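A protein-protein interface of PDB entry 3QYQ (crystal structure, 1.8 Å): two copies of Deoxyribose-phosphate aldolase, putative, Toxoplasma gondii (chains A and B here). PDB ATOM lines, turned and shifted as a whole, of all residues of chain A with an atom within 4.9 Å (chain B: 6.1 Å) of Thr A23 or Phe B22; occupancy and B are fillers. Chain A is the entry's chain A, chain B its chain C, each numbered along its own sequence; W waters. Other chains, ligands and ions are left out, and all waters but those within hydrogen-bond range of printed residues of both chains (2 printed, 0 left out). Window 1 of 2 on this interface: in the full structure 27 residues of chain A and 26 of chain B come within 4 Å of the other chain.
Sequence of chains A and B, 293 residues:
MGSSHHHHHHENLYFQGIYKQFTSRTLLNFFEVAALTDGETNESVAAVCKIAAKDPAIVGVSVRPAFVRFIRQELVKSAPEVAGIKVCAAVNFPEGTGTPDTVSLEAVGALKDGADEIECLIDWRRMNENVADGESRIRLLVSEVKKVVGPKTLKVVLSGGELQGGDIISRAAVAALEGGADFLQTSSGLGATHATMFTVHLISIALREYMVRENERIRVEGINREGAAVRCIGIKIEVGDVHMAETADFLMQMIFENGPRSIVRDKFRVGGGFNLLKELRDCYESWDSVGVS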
ATOM      1  N   TYR A  19      27.309  12.214  21.179  1.00  0.00           N
ATOM      2  CA  TYR A  19      27.173  10.768  21.419  1.00  0.00           C
ATOM      3  C   TYR A  19      28.063   9.936  20.485  1.00  0.00           C
ATOM      4  O   TYR A  19      28.644   8.932  20.898  1.00  0.00           O
ATOM      5  CB  TYR A  19      25.706  10.348  21.308  1.00  0.00           C
ATOM      6  CG  TYR A  19      24.816  11.192  22.182  1.00  0.00           C
ATOM      7  CD1 TYR A  19      24.913  11.115  23.566  1.00  0.00           C
ATOM      8  CD2 TYR A  19      23.863  12.043  21.642  1.00  0.00           C
ATOM      9  CE1 TYR A  19      24.126  11.868  24.379  1.00  0.00           C
ATOM     10  CE2 TYR A  19      23.042  12.803  22.466  1.00  0.00           C
ATOM     11  CZ  TYR A  19      23.189  12.705  23.837  1.00  0.00           C
ATOM     12  OH  TYR A  19      22.386  13.442  24.679  1.00  0.00           O
ATOM     13  N   LYS A  20      28.156  10.350  19.225  1.00  0.00           N
ATOM     14  CA  LYS A  20      29.006   9.660  18.264  1.00  0.00           C
ATOM     15  C   LYS A  20      30.459   9.838  18.689  1.00  0.00           C
ATOM     16  O   LYS A  20      31.252   8.897  18.646  1.00  0.00           O
ATOM     17  CB  LYS A  20      28.830  10.214  16.850  1.00  0.00           C
ATOM     18  CG  LYS A  20      27.461  10.000  16.248  1.00  0.00           C
ATOM     19  CD  LYS A  20      27.410  10.475  14.797  1.00  0.00           C
ATOM     20  CE  LYS A  20      28.390   9.691  13.930  1.00  0.00           C
ATOM     21  NZ  LYS A  20      28.372  10.123  12.503  1.00  0.00           N
ATOM     22  N   GLN A  21      30.783  11.048  19.129  1.00  0.00           N
ATOM     23  CA  GLN A  21      32.160  11.370  19.571  1.00  0.00           C
ATOM     24  C   GLN A  21      32.571  10.485  20.740  1.00  0.00           C
ATOM     25  O   GLN A  21      33.705   9.955  20.783  1.00  0.00           O
ATOM     26  CB  GLN A  21      32.259  12.841  19.941  1.00  0.00           C
ATOM     27  CG  GLN A  21      32.200  13.767  18.727  1.00  0.00           C
ATOM     28  CD  GLN A  21      31.914  15.230  19.056  1.00  0.00           C
ATOM     29  OE1 GLN A  21      31.473  15.565  20.144  1.00  0.00           O
ATOM     30  NE2 GLN A  21      32.124  16.111  18.068  1.00  0.00           N
ATOM     31  N   PHE A  22      31.677  10.356  21.718  1.00  0.00           N
ATOM     32  CA  PHE A  22      31.951   9.506  22.862  1.00  0.00           C
ATOM     33  C   PHE A  22      32.080   8.038  22.452  1.00  0.00           C
ATOM     34  O   PHE A  22      32.981   7.321  22.894  1.00  0.00           O
ATOM     35  CB  PHE A  22      30.910   9.663  23.979  1.00  0.00           C
ATOM     36  CG  PHE A  22      31.054   8.608  25.031  1.00  0.00           C
ATOM     37  CD1 PHE A  22      32.162   8.593  25.854  1.00  0.00           C
ATOM     38  CD2 PHE A  22      30.119   7.599  25.153  1.00  0.00           C
ATOM     39  CE1 PHE A  22      32.337   7.589  26.781  1.00  0.00           C
ATOM     40  CE2 PHE A  22      30.289   6.604  26.091  1.00  0.00           C
ATOM     41  CZ  PHE A  22      31.401   6.601  26.899  1.00  0.00           C
ATOM     42  N   THR A  23      31.182   7.578  21.597  1.00  0.00           N
ATOM     43  CA  THR A  23      31.229   6.196  21.152  1.00  0.00           C
ATOM     44  C   THR A  23      32.531   5.919  20.378  1.00  0.00           C
ATOM     45  O   THR A  23      33.150   4.865  20.551  1.00  0.00           O
ATOM     46  CB  THR A  23      29.991   5.850  20.295  1.00  0.00           C
ATOM     47  OG1 THR A  23      28.808   6.073  21.059  1.00  0.00           O
ATOM     48  CG2 THR A  23      30.044   4.406  19.853  1.00  0.00           C
ATOM     49  N   SER A  24      32.935   6.867  19.540  1.00  0.00           N
ATOM     50  CA  SER A  24      34.159   6.736  18.762  1.00  0.00           C
ATOM     51  C   SER A  24      35.376   6.674  19.686  1.00  0.00           C
ATOM     52  O   SER A  24      36.288   5.881  19.470  1.00  0.00           O
ATOM     53  CB  SER A  24      34.300   7.902  17.776  1.00  0.00           C
ATOM     54  OG  SER A  24      33.243   7.887  16.825  1.00  0.00           O
ATOM     55  N   ARG A  25      35.379   7.508  20.716  1.00  0.00           N
ATOM     56  CA  ARG A  25      36.493   7.536  21.674  1.00  0.00           C
ATOM     57  C   ARG A  25      36.582   6.195  22.413  1.00  0.00           C
ATOM     58  O   ARG A  25      37.679   5.681  22.685  1.00  0.00           O
ATOM     59  CB  ARG A  25      36.326   8.670  22.678  1.00  0.00           C
ATOM     60  CG  ARG A  25      37.432   8.717  23.732  1.00  0.00           C
ATOM     61  CD  ARG A  25      38.797   8.896  23.122  1.00  0.00           C
ATOM     62  NE  ARG A  25      39.914   8.847  24.078  1.00  0.00           N
ATOM     63  CZ  ARG A  25      40.640   7.767  24.344  1.00  0.00           C
ATOM     64  NH1 ARG A  25      40.374   6.602  23.748  1.00  0.00           N
ATOM     65  NH2 ARG A  25      41.654   7.844  25.204  1.00  0.00           N
ATOM     66  N   THR A  26      35.418   5.653  22.750  1.00  0.00           N
ATOM     67  CA  THR A  26      35.328   4.363  23.429  1.00  0.00           C
ATOM     68  C   THR A  26      35.872   3.268  22.515  1.00  0.00           C
ATOM     69  O   THR A  26      36.708   2.461  22.929  1.00  0.00           O
ATOM     70  CB  THR A  26      33.870   4.052  23.848  1.00  0.00           C
ATOM     71  OG1 THR A  26      33.421   5.010  24.808  1.00  0.00           O
ATOM     72  CG2 THR A  26      33.741   2.633  24.447  1.00  0.00           C
ATOM     73  N   LEU A  27      35.390   3.212  21.274  1.00  0.00           N
ATOM     74  CA  LEU A  27      35.857   2.205  20.326  1.00  0.00           C
ATOM     75  C   LEU A  27      37.384   2.269  20.108  1.00  0.00           C
ATOM     76  O   LEU A  27      38.035   1.226  20.042  1.00  0.00           O
ATOM     77  CB  LEU A  27      35.062   2.283  19.019  1.00  0.00           C
ATOM     78  CG  LEU A  27      33.618   1.816  19.158  1.00  0.00           C
ATOM     79  CD1 LEU A  27      32.820   2.226  17.925  1.00  0.00           C
ATOM     80  CD2 LEU A  27      33.515   0.291  19.423  1.00  0.00           C
ATOM     81  N   ALA A 248      29.156   0.057  16.772  1.00  0.00           N
ATOM     82  CA  ALA A 248      28.617   0.515  18.034  1.00  0.00           C
ATOM     83  C   ALA A 248      27.537  -0.454  18.526  1.00  0.00           C
ATOM     84  O   ALA A 248      27.410  -0.697  19.726  1.00  0.00           O
ATOM     85  CB  ALA A 248      28.061   1.944  17.889  1.00  0.00           C
ATOM     86  N   LEU A 251      29.185  -3.222  20.200  1.00  0.00           N
ATOM     87  CA  LEU A 251      29.657  -2.758  21.493  1.00  0.00           C
ATOM     88  C   LEU A 251      28.493  -2.835  22.489  1.00  0.00           C
ATOM     89  O   LEU A 251      28.652  -3.254  23.623  1.00  0.00           O
ATOM     90  CB  LEU A 251      30.147  -1.317  21.361  1.00  0.00           C
ATOM     91  CG  LEU A 251      30.564  -0.525  22.595  1.00  0.00           C
ATOM     92  CD1 LEU A 251      31.722  -1.180  23.309  1.00  0.00           C
ATOM     93  CD2 LEU A 251      30.923   0.915  22.171  1.00  0.00           C
ATOM     94  N   MET A 252      27.325  -2.414  22.027  1.00  0.00           N
ATOM     95  CA  MET A 252      26.132  -2.410  22.843  1.00  0.00           C
ATOM     96  C   MET A 252      25.718  -3.855  23.171  1.00  0.00           C
ATOM     97  O   MET A 252      25.182  -4.135  24.247  1.00  0.00           O
ATOM     98  CB  MET A 252      25.037  -1.678  22.079  1.00  0.00           C
ATOM     99  CG  MET A 252      23.882  -1.254  22.918  1.00  0.00           C
ATOM    100  SD  MET A 252      24.377  -0.099  24.224  1.00  0.00           S
ATOM    101  CE  MET A 252      22.748   0.317  24.826  1.00  0.00           C
ATOM    102  N   ILE A 255      28.105  -5.116  26.106  1.00  0.00           N
ATOM    103  CA  ILE A 255      27.687  -4.646  27.445  1.00  0.00           C
ATOM    104  C   ILE A 255      26.393  -5.284  27.891  1.00  0.00           C
ATOM    105  O   ILE A 255      26.262  -5.705  29.039  1.00  0.00           O
ATOM    106  CB  ILE A 255      27.468  -3.117  27.585  1.00  0.00           C
ATOM    107  CG1 ILE A 255      28.750  -2.407  27.967  1.00  0.00           C
ATOM    108  CG2 ILE A 255      26.560  -2.818  28.787  1.00  0.00           C
ATOM    109  CD1 ILE A 255      28.519  -0.955  28.393  1.00  0.00           C
ATOM    110  N   GLY B  17      19.928   5.833  16.568  1.00  0.00           N
ATOM    111  CA  GLY B  17      19.983   6.071  18.012  1.00  0.00           C
ATOM    112  C   GLY B  17      21.011   5.296  18.820  1.00  0.00           C
ATOM    113  O   GLY B  17      21.106   5.504  20.020  1.00  0.00           O
ATOM    114  N   ILE B  18      21.792   4.434  18.167  1.00  0.00           N
ATOM    115  CA  ILE B  18      22.771   3.597  18.869  1.00  0.00           C
ATOM    116  C   ILE B  18      23.796   4.366  19.702  1.00  0.00           C
ATOM    117  O   ILE B  18      24.142   3.949  20.802  1.00  0.00           O
ATOM    118  CB  ILE B  18      23.493   2.632  17.880  1.00  0.00           C
ATOM    119  CG1 ILE B  18      24.312   1.576  18.629  1.00  0.00           C
ATOM    120  CG2 ILE B  18      24.355   3.412  16.846  1.00  0.00           C
ATOM    121  CD1 ILE B  18      23.496   0.725  19.606  1.00  0.00           C
ATOM    122  N   TYR B  19      24.243   5.509  19.211  1.00  0.00           N
ATOM    123  CA  TYR B  19      25.253   6.269  19.949  1.00  0.00           C
ATOM    124  C   TYR B  19      24.714   6.837  21.266  1.00  0.00           C
ATOM    125  O   TYR B  19      25.386   6.778  22.305  1.00  0.00           O
ATOM    126  CB  TYR B  19      25.865   7.371  19.070  1.00  0.00           C
ATOM    127  CG  TYR B  19      26.376   6.872  17.727  1.00  0.00           C
ATOM    128  CD1 TYR B  19      27.480   6.046  17.650  1.00  0.00           C
ATOM    129  CD2 TYR B  19      25.759   7.248  16.535  1.00  0.00           C
ATOM    130  CE1 TYR B  19      27.960   5.603  16.457  1.00  0.00           C
ATOM    131  CE2 TYR B  19      26.240   6.803  15.314  1.00  0.00           C
ATOM    132  CZ  TYR B  19      27.339   5.978  15.285  1.00  0.00           C
ATOM    133  OH  TYR B  19      27.842   5.516  14.105  1.00  0.00           O
ATOM    134  N   LYS B  20      23.494   7.369  21.232  1.00  0.00           N
ATOM    135  CA  LYS B  20      22.874   7.918  22.408  1.00  0.00           C
ATOM    136  C   LYS B  20      22.537   6.781  23.363  1.00  0.00           C
ATOM    137  O   LYS B  20      22.674   6.942  24.561  1.00  0.00           O
ATOM    138  CB  LYS B  20      21.624   8.733  22.054  1.00  0.00           C
ATOM    139  CG  LYS B  20      21.109   9.566  23.224  1.00  0.00           C
ATOM    140  CD  LYS B  20      19.964  10.471  22.797  1.00  0.00           C
ATOM    141  CE  LYS B  20      19.501  11.359  23.945  1.00  0.00           C
ATOM    142  NZ  LYS B  20      18.414  12.296  23.507  1.00  0.00           N
ATOM    143  N   GLN B  21      22.109   5.629  22.830  1.00  0.00           N
ATOM    144  CA  GLN B  21      21.775   4.466  23.663  1.00  0.00           C
ATOM    145  C   GLN B  21      23.008   3.961  24.422  1.00  0.00           C
ATOM    146  O   GLN B  21      22.942   3.689  25.629  1.00  0.00           O
ATOM    147  CB  GLN B  21      21.154   3.373  22.793  1.00  0.00           C
ATOM    148  CG  GLN B  21      19.792   3.798  22.259  1.00  0.00           C
ATOM    149  CD  GLN B  21      19.329   2.970  21.074  1.00  0.00           C
ATOM    150  OE1 GLN B  21      20.110   2.242  20.468  1.00  0.00           O
ATOM    151  NE2 GLN B  21      18.061   3.150  20.683  1.00  0.00           N
ATOM    152  N   PHE B  22      24.131   3.854  23.725  1.00  0.00           N
ATOM    153  CA  PHE B  22      25.358   3.412  24.370  1.00  0.00           C
ATOM    154  C   PHE B  22      25.795   4.431  25.412  1.00  0.00           C
ATOM    155  O   PHE B  22      26.233   4.073  26.507  1.00  0.00           O
ATOM    156  CB  PHE B  22      26.489   3.130  23.377  1.00  0.00           C
ATOM    157  CG  PHE B  22      27.775   2.788  24.065  1.00  0.00           C
ATOM    158  CD1 PHE B  22      27.937   1.550  24.662  1.00  0.00           C
ATOM    159  CD2 PHE B  22      28.800   3.709  24.155  1.00  0.00           C
ATOM    160  CE1 PHE B  22      29.092   1.235  25.347  1.00  0.00           C
ATOM    161  CE2 PHE B  22      29.979   3.387  24.844  1.00  0.00           C
ATOM    162  CZ  PHE B  22      30.111   2.156  25.427  1.00  0.00           C
ATOM    163  N   THR B  23      25.689   5.709  25.078  1.00  0.00           N
ATOM    164  CA  THR B  23      26.076   6.744  26.030  1.00  0.00           C
ATOM    165  C   THR B  23      25.201   6.640  27.305  1.00  0.00           C
ATOM    166  O   THR B  23      25.706   6.718  28.420  1.00  0.00           O
ATOM    167  CB  THR B  23      25.982   8.127  25.406  1.00  0.00           C
ATOM    168  OG1 THR B  23      26.782   8.179  24.211  1.00  0.00           O
ATOM    169  CG2 THR B  23      26.448   9.206  26.404  1.00  0.00           C
ATOM    170  N   SER B  24      23.901   6.432  27.114  1.00  0.00           N
ATOM    171  CA  SER B  24      22.970   6.312  28.225  1.00  0.00           C
ATOM    172  C   SER B  24      23.323   5.134  29.124  1.00  0.00           C
ATOM    173  O   SER B  24      23.298   5.255  30.349  1.00  0.00           O
ATOM    174  CB  SER B  24      21.544   6.139  27.705  1.00  0.00           C
ATOM    175  OG  SER B  24      21.055   7.341  27.140  1.00  0.00           O
ATOM    176  N   ARG B  25      23.647   3.995  28.516  1.00  0.00           N
ATOM    177  CA  ARG B  25      24.000   2.789  29.274  1.00  0.00           C
ATOM    178  C   ARG B  25      25.234   3.047  30.124  1.00  0.00           C
ATOM    179  O   ARG B  25      25.304   2.654  31.290  1.00  0.00           O
ATOM    180  CB  ARG B  25      24.257   1.590  28.361  1.00  0.00           C
ATOM    181  CG  ARG B  25      24.687   0.335  29.133  1.00  0.00           C
ATOM    182  CD  ARG B  25      23.585  -0.133  30.068  1.00  0.00           C
ATOM    183  NE  ARG B  25      23.966  -1.233  30.942  1.00  0.00           N
ATOM    184  CZ  ARG B  25      24.436  -1.088  32.178  1.00  0.00           C
ATOM    185  NH1 ARG B  25      24.598   0.118  32.707  1.00  0.00           N
ATOM    186  NH2 ARG B  25      24.723  -2.161  32.904  1.00  0.00           N
ATOM    187  N   THR B  26      26.189   3.732  29.517  1.00  0.00           N
ATOM    188  CA  THR B  26      27.425   4.088  30.172  1.00  0.00           C
ATOM    189  C   THR B  26      27.150   4.998  31.370  1.00  0.00           C
ATOM    190  O   THR B  26      27.621   4.727  32.478  1.00  0.00           O
ATOM    191  CB  THR B  26      28.387   4.770  29.197  1.00  0.00           C
ATOM    192  OG1 THR B  26      28.763   3.845  28.166  1.00  0.00           O
ATOM    193  CG2 THR B  26      29.642   5.221  29.924  1.00  0.00           C
ATOM    194  N   LEU B  27      26.383   6.062  31.160  1.00  0.00           N
ATOM    195  CA  LEU B  27      26.060   6.998  32.240  1.00  0.00           C
ATOM    196  C   LEU B  27      25.294   6.304  33.365  1.00  0.00           C
ATOM    197  O   LEU B  27      25.556   6.567  34.533  1.00  0.00           O
ATOM    198  CB  LEU B  27      25.336   8.231  31.710  1.00  0.00           C
ATOM    199  CG  LEU B  27      26.205   9.130  30.831  1.00  0.00           C
ATOM    200  CD1 LEU B  27      25.359  10.146  30.103  1.00  0.00           C
ATOM    201  CD2 LEU B  27      27.336   9.803  31.673  1.00  0.00           C
ATOM    202  N   MET B 252      33.113  13.154  28.312  1.00  0.00           N
ATOM    203  CA  MET B 252      34.246  13.316  27.391  1.00  0.00           C
ATOM    204  C   MET B 252      35.384  14.096  28.048  1.00  0.00           C
ATOM    205  O   MET B 252      36.548  13.786  27.830  1.00  0.00           O
ATOM    206  CB  MET B 252      33.809  13.973  26.072  1.00  0.00           C
ATOM    207  CG  MET B 252      33.006  13.019  25.212  1.00  0.00           C
ATOM    208  SD  MET B 252      34.082  11.775  24.487  1.00  0.00           S
ATOM    209  CE  MET B 252      34.851  12.675  23.133  1.00  0.00           C
ATOM    210  N   CYS B 283      16.160   6.308  27.234  1.00  0.00           N
ATOM    211  CA  CYS B 283      17.072   6.199  26.102  1.00  0.00           C
ATOM    212  C   CYS B 283      17.612   4.780  25.981  1.00  0.00           C
ATOM    213  O   CYS B 283      17.477   4.143  24.931  1.00  0.00           O
ATOM    214  CB  CYS B 283      18.220   7.201  26.221  1.00  0.00           C
ATOM    215  SG  CYS B 283      19.366   7.130  24.821  1.00  0.00           S
HETATM  216  O   HOH W   1      20.392  14.756  23.747  1.00  0.00           O
HETATM  217  O   HOH W   2      24.605  -4.322  30.913  1.00  0.00           O
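Of the 13 printed residues of chain A, 10 touch a printed residue of chain B.
Hydrophobic or aromatic side chains of chain A that line the printed part of chain B: Tyr A19, Phe A22, Ala A248, Leu A251, Met A252 and Ile A255.
Along chain A the printed residues that touch a printed residue of chain B span positions 19 to 255.
Of the 13 printed residues of chain B, 9 touch a printed residue of chain A.
Hydrophobic or aromatic side chains of chain B that line the printed part of chain A: Ile B18, Tyr B19, Phe B22 and Met B252.
Among the printed residues, no Asp or Glu carboxylate lies within 4 Å of a Lys or Arg side-chain nitrogen of the other chain.
Tyr A19 touches its own counterpart, Tyr B19.
Tyr A19 touches Thr B23, and with the chains exchanged Thr A23 touches Tyr B19.
Gln A21 touches Met B252, and with the chains exchanged Met A252 touches Gln B21.
Phe A22 touches Thr B26, and with the chains exchanged Thr A26 touches Phe B22.
Positions printed for both chains: 19, 20, 21, 22, 23, 24, 25, 26, 27 and 252.
Of the 20 pairs that touch across the chains among the printed residues, 14 have their exchanged pair printed and touching as well.
Among the printed residues, merely in contact across the chains: Tyr A19 with Tyr B19 (3.6 Å), Tyr A19 with Lys B20 (3.6 Å), Tyr A19 with Thr B23 (3.5 Å), Lys A20 with Tyr B19 (3.2 Å), Gln A21 with Met B252 (3.8 Å), Phe A22 with Phe B22 (3.5 Å), Phe A22 with Thr B23 (3.5 Å), Phe A22 with Thr B26 (3.8 Å), Phe A22 with Met B252 (3.5 Å), Thr A23 with Tyr B19 (3.7 Å), Thr A23 with Phe B22 (3.9 Å), Thr A26 with Phe B22 (3.8 Å), Ala A248 with Ile B18 (3.8 Å), Ala A248 with Tyr B19 (3.9 Å), Leu A251 with Phe B22 (3.6 Å), Met A252 with Ile B18 (3.8 Å), Met A252 with Gln B21 (3.5 Å), Met A252 with Phe B22 (3.6 Å), Ile A255 with Phe B22 (3.8 Å) and Ile A255 with Arg B25 (3.7 Å).
Printed residues of chain B within 4 Å of Lys A20: Tyr B19.
Thr A23 touches just these residues of chain B: Tyr B19 and Phe B22.
Leu A27 touches none of the printed residues of chain B.
Of the printed residues of chain B, Ala A248 touches Ile B18 (3.8 Å) and Tyr B19 (3.9 Å).
Of the printed residues of chain B, Ile A255 touches Phe B22 and Arg B25.
Of the printed residues of chain A, Phe B22 touches Phe A22, Thr A23, Thr A26, Leu A251, Met A252 and Ile A255.
Printed residues of chain A within 4 Å of Thr B23: Tyr A19 (3.5 Å) and Phe A22 (3.5 Å).
Of the printed residues of chain A, Arg B25 touches Ile A255.
Leu B27 touches none of the printed residues of chain A.
The nearest residue of chain B that does not touch Thr A23 is Thr B23 (4.3 Å).
The nearest printed residue of chain A that does not touch Thr B23 is Thr A23 (4.3 Å).
The backbone carbonyl oxygen of Tyr A19 lies within hydrogen-bond range of the side-chain hydroxyl of Thr A23, 2.9 Å away.
The backbone carbonyl oxygen of Gly B17 lies close to the side-chain amide oxygen of Gln B21 (3.4 Å).
The side-chain hydroxyl (OG1) of Thr B23 is in hydrogen-bond range of the backbone carbonyl oxygen (O) of Tyr B19 (2.7 Å).
O of Lys B20 is in hydrogen-bond range of OG of Ser B24.
The side-chain sulfur of Cys B283 is in hydrogen-bond range of the backbone carbonyl oxygen of Lys B20, at 3.3 Å.
The side-chain hydroxyl (OG1) of Thr B26 is in hydrogen-bond range of the backbone carbonyl oxygen (O) of Phe B22 (3.0 Å).
Water W1 lies within hydrogen-bond range of the side-chain hydroxyl of Tyr A19 and the side-chain amino group of Lys B20.
Water W2 bridges O of Ile A255 (2.9 Å) and NH2 of Arg B25 (2.9 Å).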
